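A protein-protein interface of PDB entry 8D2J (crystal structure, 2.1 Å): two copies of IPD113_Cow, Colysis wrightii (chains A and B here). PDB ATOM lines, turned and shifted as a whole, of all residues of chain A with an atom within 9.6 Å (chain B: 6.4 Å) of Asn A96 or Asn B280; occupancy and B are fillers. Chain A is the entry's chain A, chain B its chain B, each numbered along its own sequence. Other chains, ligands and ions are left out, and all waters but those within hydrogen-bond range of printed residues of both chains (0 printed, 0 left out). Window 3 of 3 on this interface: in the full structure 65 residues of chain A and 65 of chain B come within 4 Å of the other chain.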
ATOM      1  N   GLU A  26     -11.050 -12.969  15.530  1.00  0.00           N
ATOM      2  CA  GLU A  26     -10.364 -13.012  14.201  1.00  0.00           C
ATOM      3  C   GLU A  26     -10.596 -14.383  13.553  1.00  0.00           C
ATOM      4  O   GLU A  26      -9.843 -15.320  13.872  1.00  0.00           O
ATOM      5  CB  GLU A  26      -8.871 -12.719  14.367  1.00  0.00           C
ATOM      6  N   ASP A  28     -10.771 -17.399  10.669  1.00  0.00           N
ATOM      7  CA  ASP A  28      -9.992 -17.925   9.515  1.00  0.00           C
ATOM      8  C   ASP A  28     -10.708 -17.490   8.235  1.00  0.00           C
ATOM      9  O   ASP A  28     -11.897 -17.754   8.079  1.00  0.00           O
ATOM     10  CB  ASP A  28      -9.829 -19.446   9.607  1.00  0.00           C
ATOM     11  CG  ASP A  28      -8.872 -20.049   8.589  1.00  0.00           C
ATOM     12  OD1 ASP A  28      -8.840 -19.557   7.444  1.00  0.00           O
ATOM     13  OD2 ASP A  28      -8.170 -21.015   8.947  1.00  0.00           O
ATOM     14  N   PRO A  29     -10.023 -16.791   7.298  1.00  0.00           N
ATOM     15  CA  PRO A  29     -10.675 -16.263   6.095  1.00  0.00           C
ATOM     16  C   PRO A  29     -11.426 -17.285   5.226  1.00  0.00           C
ATOM     17  O   PRO A  29     -12.303 -16.867   4.495  1.00  0.00           O
ATOM     18  CB  PRO A  29      -9.508 -15.675   5.285  1.00  0.00           C
ATOM     19  CG  PRO A  29      -8.469 -15.330   6.325  1.00  0.00           C
ATOM     20  CD  PRO A  29      -8.599 -16.420   7.367  1.00  0.00           C
ATOM     21  N   GLU A  59     -11.154 -31.585   4.652  1.00  0.00           N
ATOM     22  CA  GLU A  59     -10.164 -31.383   5.750  1.00  0.00           C
ATOM     23  C   GLU A  59     -10.092 -32.635   6.634  1.00  0.00           C
ATOM     24  O   GLU A  59      -8.977 -32.979   7.074  1.00  0.00           O
ATOM     25  CB  GLU A  59     -10.505 -30.147   6.587  1.00  0.00           C
ATOM     26  CG  GLU A  59      -9.738 -28.905   6.173  1.00  0.00           C
ATOM     27  CD  GLU A  59      -8.239 -28.995   6.404  1.00  0.00           C
ATOM     28  OE1 GLU A  59      -7.816 -28.975   7.579  1.00  0.00           O
ATOM     29  OE2 GLU A  59      -7.499 -29.113   5.407  1.00  0.00           O
ATOM     30  N   ASP A  62      -7.540 -34.842   5.250  1.00  0.00           N
ATOM     31  CA  ASP A  62      -6.392 -33.989   4.839  1.00  0.00           C
ATOM     32  C   ASP A  62      -5.218 -34.896   4.442  1.00  0.00           C
ATOM     33  O   ASP A  62      -4.802 -34.826   3.270  1.00  0.00           O
ATOM     34  CB  ASP A  62      -6.021 -32.986   5.935  1.00  0.00           C
ATOM     35  CG  ASP A  62      -4.912 -32.017   5.553  1.00  0.00           C
ATOM     36  OD1 ASP A  62      -4.697 -31.815   4.344  1.00  0.00           O
ATOM     37  OD2 ASP A  62      -4.267 -31.476   6.474  1.00  0.00           O
ATOM     38  N   ARG A  66      -3.326 -35.559   0.786  1.00  0.00           N
ATOM     39  CA  ARG A  66      -1.884 -35.212   0.641  1.00  0.00           C
ATOM     40  C   ARG A  66      -1.127 -36.373  -0.016  1.00  0.00           C
ATOM     41  O   ARG A  66      -0.333 -36.111  -0.939  1.00  0.00           O
ATOM     42  CB  ARG A  66      -1.250 -34.901   1.998  1.00  0.00           C
ATOM     43  CG  ARG A  66      -1.781 -33.642   2.665  1.00  0.00           C
ATOM     44  CD  ARG A  66      -0.910 -33.285   3.848  1.00  0.00           C
ATOM     45  NE  ARG A  66      -1.473 -32.224   4.667  1.00  0.00           N
ATOM     46  CZ  ARG A  66      -0.795 -31.525   5.573  1.00  0.00           C
ATOM     47  NH1 ARG A  66       0.494 -31.754   5.770  1.00  0.00           N
ATOM     48  NH2 ARG A  66      -1.410 -30.588   6.275  1.00  0.00           N
ATOM     49  N   ILE A  89       6.873 -32.407  -1.194  1.00  0.00           N
ATOM     50  CA  ILE A  89       7.409 -31.719   0.021  1.00  0.00           C
ATOM     51  C   ILE A  89       6.414 -30.638   0.457  1.00  0.00           C
ATOM     52  O   ILE A  89       6.119 -30.566   1.665  1.00  0.00           O
ATOM     53  CB  ILE A  89       8.822 -31.153  -0.237  1.00  0.00           C
ATOM     54  CG1 ILE A  89       9.847 -32.273  -0.437  1.00  0.00           C
ATOM     55  CG2 ILE A  89       9.243 -30.203   0.878  1.00  0.00           C
ATOM     56  CD1 ILE A  89      11.103 -31.842  -1.158  1.00  0.00           C
ATOM     57  N   GLY A  90       5.913 -29.844  -0.495  1.00  0.00           N
ATOM     58  CA  GLY A  90       4.904 -28.790  -0.267  1.00  0.00           C
ATOM     59  C   GLY A  90       3.642 -29.338   0.380  1.00  0.00           C
ATOM     60  O   GLY A  90       3.116 -28.677   1.291  1.00  0.00           O
ATOM     61  N   LEU A  91       3.171 -30.505  -0.071  1.00  0.00           N
ATOM     62  CA  LEU A  91       1.962 -31.180   0.476  1.00  0.00           C
ATOM     63  C   LEU A  91       2.269 -31.730   1.875  1.00  0.00           C
ATOM     64  O   LEU A  91       1.475 -31.464   2.794  1.00  0.00           O
ATOM     65  CB  LEU A  91       1.520 -32.300  -0.475  1.00  0.00           C
ATOM     66  CG  LEU A  91       1.005 -31.852  -1.843  1.00  0.00           C
ATOM     67  CD1 LEU A  91       0.867 -33.039  -2.785  1.00  0.00           C
ATOM     68  CD2 LEU A  91      -0.321 -31.119  -1.721  1.00  0.00           C
ATOM     69  N   PHE A  92       3.384 -32.450   2.029  1.00  0.00           N
ATOM     70  CA  PHE A  92       3.741 -33.218   3.253  1.00  0.00           C
ATOM     71  C   PHE A  92       4.259 -32.282   4.355  1.00  0.00           C
ATOM     72  O   PHE A  92       3.989 -32.564   5.541  1.00  0.00           O
ATOM     73  CB  PHE A  92       4.767 -34.308   2.928  1.00  0.00           C
ATOM     74  CG  PHE A  92       4.193 -35.604   2.409  1.00  0.00           C
ATOM     75  CD1 PHE A  92       4.786 -36.815   2.736  1.00  0.00           C
ATOM     76  CD2 PHE A  92       3.064 -35.624   1.602  1.00  0.00           C
ATOM     77  CE1 PHE A  92       4.272 -38.011   2.259  1.00  0.00           C
ATOM     78  CE2 PHE A  92       2.550 -36.823   1.128  1.00  0.00           C
ATOM     79  CZ  PHE A  92       3.154 -38.012   1.457  1.00  0.00           C
ATOM     80  N   TRP A  93       4.989 -31.221   3.989  1.00  0.00           N
ATOM     81  CA  TRP A  93       5.614 -30.267   4.947  1.00  0.00           C
ATOM     82  C   TRP A  93       5.338 -28.827   4.520  1.00  0.00           C
ATOM     83  O   TRP A  93       6.264 -28.077   4.222  1.00  0.00           O
ATOM     84  CB  TRP A  93       7.114 -30.561   5.078  1.00  0.00           C
ATOM     85  CG  TRP A  93       7.379 -31.934   5.610  1.00  0.00           C
ATOM     86  CD1 TRP A  93       7.330 -32.329   6.914  1.00  0.00           C
ATOM     87  CD2 TRP A  93       7.685 -33.113   4.845  1.00  0.00           C
ATOM     88  NE1 TRP A  93       7.600 -33.667   7.017  1.00  0.00           N
ATOM     89  CE2 TRP A  93       7.826 -34.176   5.765  1.00  0.00           C
ATOM     90  CE3 TRP A  93       7.872 -33.373   3.484  1.00  0.00           C
ATOM     91  CZ2 TRP A  93       8.138 -35.473   5.362  1.00  0.00           C
ATOM     92  CZ3 TRP A  93       8.180 -34.657   3.086  1.00  0.00           C
ATOM     93  CH2 TRP A  93       8.310 -35.691   4.014  1.00  0.00           C
ATOM     94  N   PRO A  94       4.056 -28.393   4.504  1.00  0.00           N
ATOM     95  CA  PRO A  94       3.705 -27.011   4.173  1.00  0.00           C
ATOM     96  C   PRO A  94       4.090 -26.030   5.292  1.00  0.00           C
ATOM     97  O   PRO A  94       4.333 -26.469   6.399  1.00  0.00           O
ATOM     98  CB  PRO A  94       2.181 -27.063   4.003  1.00  0.00           C
ATOM     99  CG  PRO A  94       1.757 -28.188   4.917  1.00  0.00           C
ATOM    100  CD  PRO A  94       2.871 -29.208   4.817  1.00  0.00           C
ATOM    101  N   ALA A  95       4.122 -24.733   4.971  1.00  0.00           N
ATOM    102  CA  ALA A  95       4.564 -23.640   5.871  1.00  0.00           C
ATOM    103  C   ALA A  95       3.437 -23.248   6.835  1.00  0.00           C
ATOM    104  O   ALA A  95       3.745 -22.926   8.000  1.00  0.00           O
ATOM    105  CB  ALA A  95       5.020 -22.457   5.051  1.00  0.00           C
ATOM    106  N   ASN A  96       2.184 -23.284   6.367  1.00  0.00           N
ATOM    107  CA  ASN A  96       1.007 -22.687   7.056  1.00  0.00           C
ATOM    108  C   ASN A  96       0.059 -23.774   7.582  1.00  0.00           C
ATOM    109  O   ASN A  96      -0.961 -23.408   8.201  1.00  0.00           O
ATOM    110  CB  ASN A  96       0.269 -21.721   6.126  1.00  0.00           C
ATOM    111  CG  ASN A  96       1.091 -20.493   5.798  1.00  0.00           C
ATOM    112  OD1 ASN A  96       1.655 -19.862   6.690  1.00  0.00           O
ATOM    113  ND2 ASN A  96       1.164 -20.145   4.523  1.00  0.00           N
ATOM    114  N   LYS A  97       0.370 -25.056   7.362  1.00  0.00           N
ATOM    115  CA  LYS A  97      -0.504 -26.184   7.779  1.00  0.00           C
ATOM    116  C   LYS A  97       0.298 -27.198   8.599  1.00  0.00           C
ATOM    117  O   LYS A  97       1.544 -27.141   8.591  1.00  0.00           O
ATOM    118  CB  LYS A  97      -1.147 -26.855   6.560  1.00  0.00           C
ATOM    119  CG  LYS A  97      -2.059 -25.962   5.730  1.00  0.00           C
ATOM    120  CD  LYS A  97      -3.002 -26.732   4.828  1.00  0.00           C
ATOM    121  CE  LYS A  97      -4.173 -27.336   5.576  1.00  0.00           C
ATOM    122  NZ  LYS A  97      -5.050 -28.125   4.678  1.00  0.00           N
ATOM    123  N   VAL A  98      -0.425 -28.082   9.289  1.00  0.00           N
ATOM    124  CA  VAL A  98       0.111 -29.261  10.031  1.00  0.00           C
ATOM    125  C   VAL A  98       0.940 -30.107   9.052  1.00  0.00           C
ATOM    126  O   VAL A  98       0.666 -30.037   7.840  1.00  0.00           O
ATOM    127  CB  VAL A  98      -1.055 -30.046  10.665  1.00  0.00           C
ATOM    128  CG1 VAL A  98      -0.650 -31.435  11.106  1.00  0.00           C
ATOM    129  CG2 VAL A  98      -1.678 -29.290  11.828  1.00  0.00           C
ATOM    130  N   ASP A  99       1.937 -30.852   9.545  1.00  0.00           N
ATOM    131  CA  ASP A  99       2.782 -31.747   8.706  1.00  0.00           C
ATOM    132  C   ASP A  99       2.029 -33.062   8.476  1.00  0.00           C
ATOM    133  O   ASP A  99       0.954 -33.246   9.082  1.00  0.00           O
ATOM    134  CB  ASP A  99       4.179 -31.946   9.303  1.00  0.00           C
ATOM    135  CG  ASP A  99       4.267 -32.887  10.494  1.00  0.00           C
ATOM    136  OD1 ASP A  99       5.325 -32.887  11.151  1.00  0.00           O
ATOM    137  OD2 ASP A  99       3.295 -33.619  10.750  1.00  0.00           O
ATOM    138  N   CYS B 256       9.842 -24.819   8.101  1.00  0.00           N
ATOM    139  CA  CYS B 256       9.528 -24.083   9.354  1.00  0.00           C
ATOM    140  C   CYS B 256       8.094 -24.426   9.777  1.00  0.00           C
ATOM    141  O   CYS B 256       7.153 -23.832   9.214  1.00  0.00           O
ATOM    142  CB  CYS B 256       9.701 -22.578   9.175  1.00  0.00           C
ATOM    143  SG  CYS B 256      11.436 -22.052   9.150  1.00  0.00           S
ATOM    144  N   PRO B 258       4.622 -24.476  11.700  1.00  0.00           N
ATOM    145  CA  PRO B 258       3.901 -23.364  12.318  1.00  0.00           C
ATOM    146  C   PRO B 258       3.444 -23.678  13.751  1.00  0.00           C
ATOM    147  O   PRO B 258       3.434 -24.841  14.121  1.00  0.00           O
ATOM    148  CB  PRO B 258       2.690 -23.204  11.388  1.00  0.00           C
ATOM    149  CG  PRO B 258       2.399 -24.617  10.927  1.00  0.00           C
ATOM    150  CD  PRO B 258       3.756 -25.288  10.829  1.00  0.00           C
ATOM    151  N   ASP B 259       3.088 -22.638  14.513  1.00  0.00           N
ATOM    152  CA  ASP B 259       2.413 -22.760  15.832  1.00  0.00           C
ATOM    153  C   ASP B 259       1.058 -23.443  15.619  1.00  0.00           C
ATOM    154  O   ASP B 259       0.380 -23.107  14.625  1.00  0.00           O
ATOM    155  CB  ASP B 259       2.203 -21.397  16.502  1.00  0.00           C
ATOM    156  CG  ASP B 259       3.478 -20.687  16.928  1.00  0.00           C
ATOM    157  OD1 ASP B 259       4.536 -21.340  16.960  1.00  0.00           O
ATOM    158  OD2 ASP B 259       3.399 -19.482  17.229  1.00  0.00           O
ATOM    159  N   VAL B 260       0.687 -24.364  16.509  1.00  0.00           N
ATOM    160  CA  VAL B 260      -0.657 -25.013  16.531  1.00  0.00           C
ATOM    161  C   VAL B 260      -1.248 -24.836  17.934  1.00  0.00           C
ATOM    162  O   VAL B 260      -0.587 -25.242  18.906  1.00  0.00           O
ATOM    163  CB  VAL B 260      -0.593 -26.497  16.121  1.00  0.00           C
ATOM    164  CG1 VAL B 260      -1.980 -27.055  15.840  1.00  0.00           C
ATOM    165  CG2 VAL B 260       0.318 -26.721  14.920  1.00  0.00           C
ATOM    166  N   SER B 261      -2.435 -24.225  18.019  1.00  0.00           N
ATOM    167  CA  SER B 261      -3.231 -24.054  19.262  1.00  0.00           C
ATOM    168  C   SER B 261      -4.328 -25.121  19.301  1.00  0.00           C
ATOM    169  O   SER B 261      -5.036 -25.268  18.286  1.00  0.00           O
ATOM    170  CB  SER B 261      -3.809 -22.669  19.349  1.00  0.00           C
ATOM    171  OG  SER B 261      -2.777 -21.695  19.405  1.00  0.00           O
ATOM    172  N   ALA B 278      -6.047 -25.033  15.527  1.00  0.00           N
ATOM    173  CA  ALA B 278      -5.845 -23.971  14.517  1.00  0.00           C
ATOM    174  C   ALA B 278      -4.346 -23.692  14.377  1.00  0.00           C
ATOM    175  O   ALA B 278      -3.691 -23.437  15.410  1.00  0.00           O
ATOM    176  CB  ALA B 278      -6.605 -22.730  14.909  1.00  0.00           C
ATOM    177  N   THR B 279      -3.833 -23.757  13.145  1.00  0.00           N
ATOM    178  CA  THR B 279      -2.410 -23.500  12.799  1.00  0.00           C
ATOM    179  C   THR B 279      -2.195 -21.986  12.670  1.00  0.00           C
ATOM    180  O   THR B 279      -3.181 -21.271  12.401  1.00  0.00           O
ATOM    181  CB  THR B 279      -2.014 -24.249  11.521  1.00  0.00           C
ATOM    182  OG1 THR B 279      -2.769 -23.695  10.443  1.00  0.00           O
ATOM    183  CG2 THR B 279      -2.259 -25.739  11.610  1.00  0.00           C
ATOM    184  N   ASN B 280      -0.952 -21.531  12.863  1.00  0.00           N
ATOM    185  CA  ASN B 280      -0.534 -20.105  12.772  1.00  0.00           C
ATOM    186  C   ASN B 280      -1.306 -19.276  13.807  1.00  0.00           C
ATOM    187  O   ASN B 280      -1.672 -18.127  13.495  1.00  0.00           O
ATOM    188  CB  ASN B 280      -0.696 -19.563  11.348  1.00  0.00           C
ATOM    189  CG  ASN B 280       0.255 -20.212  10.364  1.00  0.00           C
ATOM    190  OD1 ASN B 280      -0.174 -20.823   9.388  1.00  0.00           O
ATOM    191  ND2 ASN B 280       1.548 -20.091  10.615  1.00  0.00           N
ATOM    192  N   ARG B 281      -1.542 -19.850  14.990  1.00  0.00           N
ATOM    193  CA  ARG B 281      -2.131 -19.164  16.171  1.00  0.00           C
ATOM    194  C   ARG B 281      -1.443 -19.695  17.433  1.00  0.00           C
ATOM    195  O   ARG B 281      -1.278 -20.927  17.541  1.00  0.00           O
ATOM    196  CB  ARG B 281      -3.649 -19.375  16.228  1.00  0.00           C
ATOM    197  CG  ARG B 281      -4.431 -18.568  15.201  1.00  0.00           C
ATOM    198  CD  ARG B 281      -5.925 -18.817  15.294  1.00  0.00           C
ATOM    199  NE  ARG B 281      -6.654 -18.407  14.097  1.00  0.00           N
ATOM    200  CZ  ARG B 281      -7.343 -17.274  13.953  1.00  0.00           C
ATOM    201  NH1 ARG B 281      -7.417 -16.386  14.934  1.00  0.00           N
ATOM    202  NH2 ARG B 281      -7.966 -17.031  12.812  1.00  0.00           N
ATOM    203  N   ASN B 282      -1.044 -18.789  18.330  1.00  0.00           N
ATOM    204  CA  ASN B 282      -0.407 -19.093  19.639  1.00  0.00           C
ATOM    205  C   ASN B 282      -1.318 -18.548  20.745  1.00  0.00           C
ATOM    206  O   ASN B 282      -1.151 -17.369  21.120  1.00  0.00           O
ATOM    207  CB  ASN B 282       1.011 -18.519  19.708  1.00  0.00           C
ATOM    208  CG  ASN B 282       1.678 -18.711  21.054  1.00  0.00           C
ATOM    209  OD1 ASN B 282       1.424 -19.690  21.750  1.00  0.00           O
ATOM    210  ND2 ASN B 282       2.541 -17.779  21.424  1.00  0.00           N
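Printed residues of chain B within 4 Å of Glu A26: Arg B281. Leu A91 touches none of the printed residues of chain B. Trp A93 touches none of the printed residues of chain B. Printed residues of chain B within 4 Å of Ala A95: Cys B256 and Pro B258. Asn A96 touches just these residues of chain B: Thr B279 and Asn B280. Printed residues of chain B within 4 Å of Val A98: Thr B279 (3.6 Å). Of the printed residues of chain A, Cys B256 touches Ala A95 (3.7 Å). Of chain A, only Asn A96 (2.9 Å) and Val A98 (3.6 Å) come within 4 Å of Thr B279. Printed residues of chain A within 4 Å of Arg B281: Glu A26 (2.8 Å) and Asp A28 (3.5 Å). The nearest printed residue of chain A that does not touch Arg B281 is Pro A29 (5.5 Å).
No position is printed for both chains. Of the 8 pairs that touch across the chains among the printed residues, none has its exchanged pair printed and touching as well.
Among the printed residues, merely in contact across the chains: Asp A28 with Arg B281 (3.5 Å), Ala A95 with Cys B256 (3.7 Å), Ala A95 with Pro B258 (3.6 Å), Lys A97 with Pro B258 (3.5 Å) and Val A98 with Thr B279 (3.6 Å).
The side-chain hydroxyl (OG1) of Thr B279 lies within hydrogen-bond range of the backbone carbonyl oxygen (O) of Asn A96 (2.9 Å). The guanidinium group (NH2) of Arg B281 lies within hydrogen-bond range of the backbone carbonyl oxygen (O) of Glu A26 (2.8 Å). The side-chain amide oxygen of Asn B280 sits close to the backbone carbonyl oxygen of Asn A96 (3.0 Å).
Of the 10 printed residues of chain B, 5 touch a printed residue of chain A. Of the 17 printed residues of chain A, 6 touch a printed residue of chain B. Hydrophobic or aromatic side chains of chain A within 4 Å of the printed part of chain B: Val A98. Among the printed residues, 8 pairs touch across the chains. Among the printed residues, no Asp or Glu carboxylate lies within 4 Å of a Lys or Arg side-chain nitrogen of the other chain.
The guanidinium group of Arg A66 sits at hydrogen-bond distance from the backbone carbonyl oxygen of Val A98 (2.7 Å). NZ of Lys A97 lies within salt-bridge range of OE2 of Glu A59, at 2.7 Å. O of Asp B259 lies within hydrogen-bond range of N of Asn B280 (2.7 Å). OD1 of Asp A62 is in salt-bridge range of NZ of Lys A97 (3.7 Å). The side-chain hydroxyl (OG) of Ser B261 sits at hydrogen-bond distance from the backbone carbonyl oxygen (O) of Arg B281.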
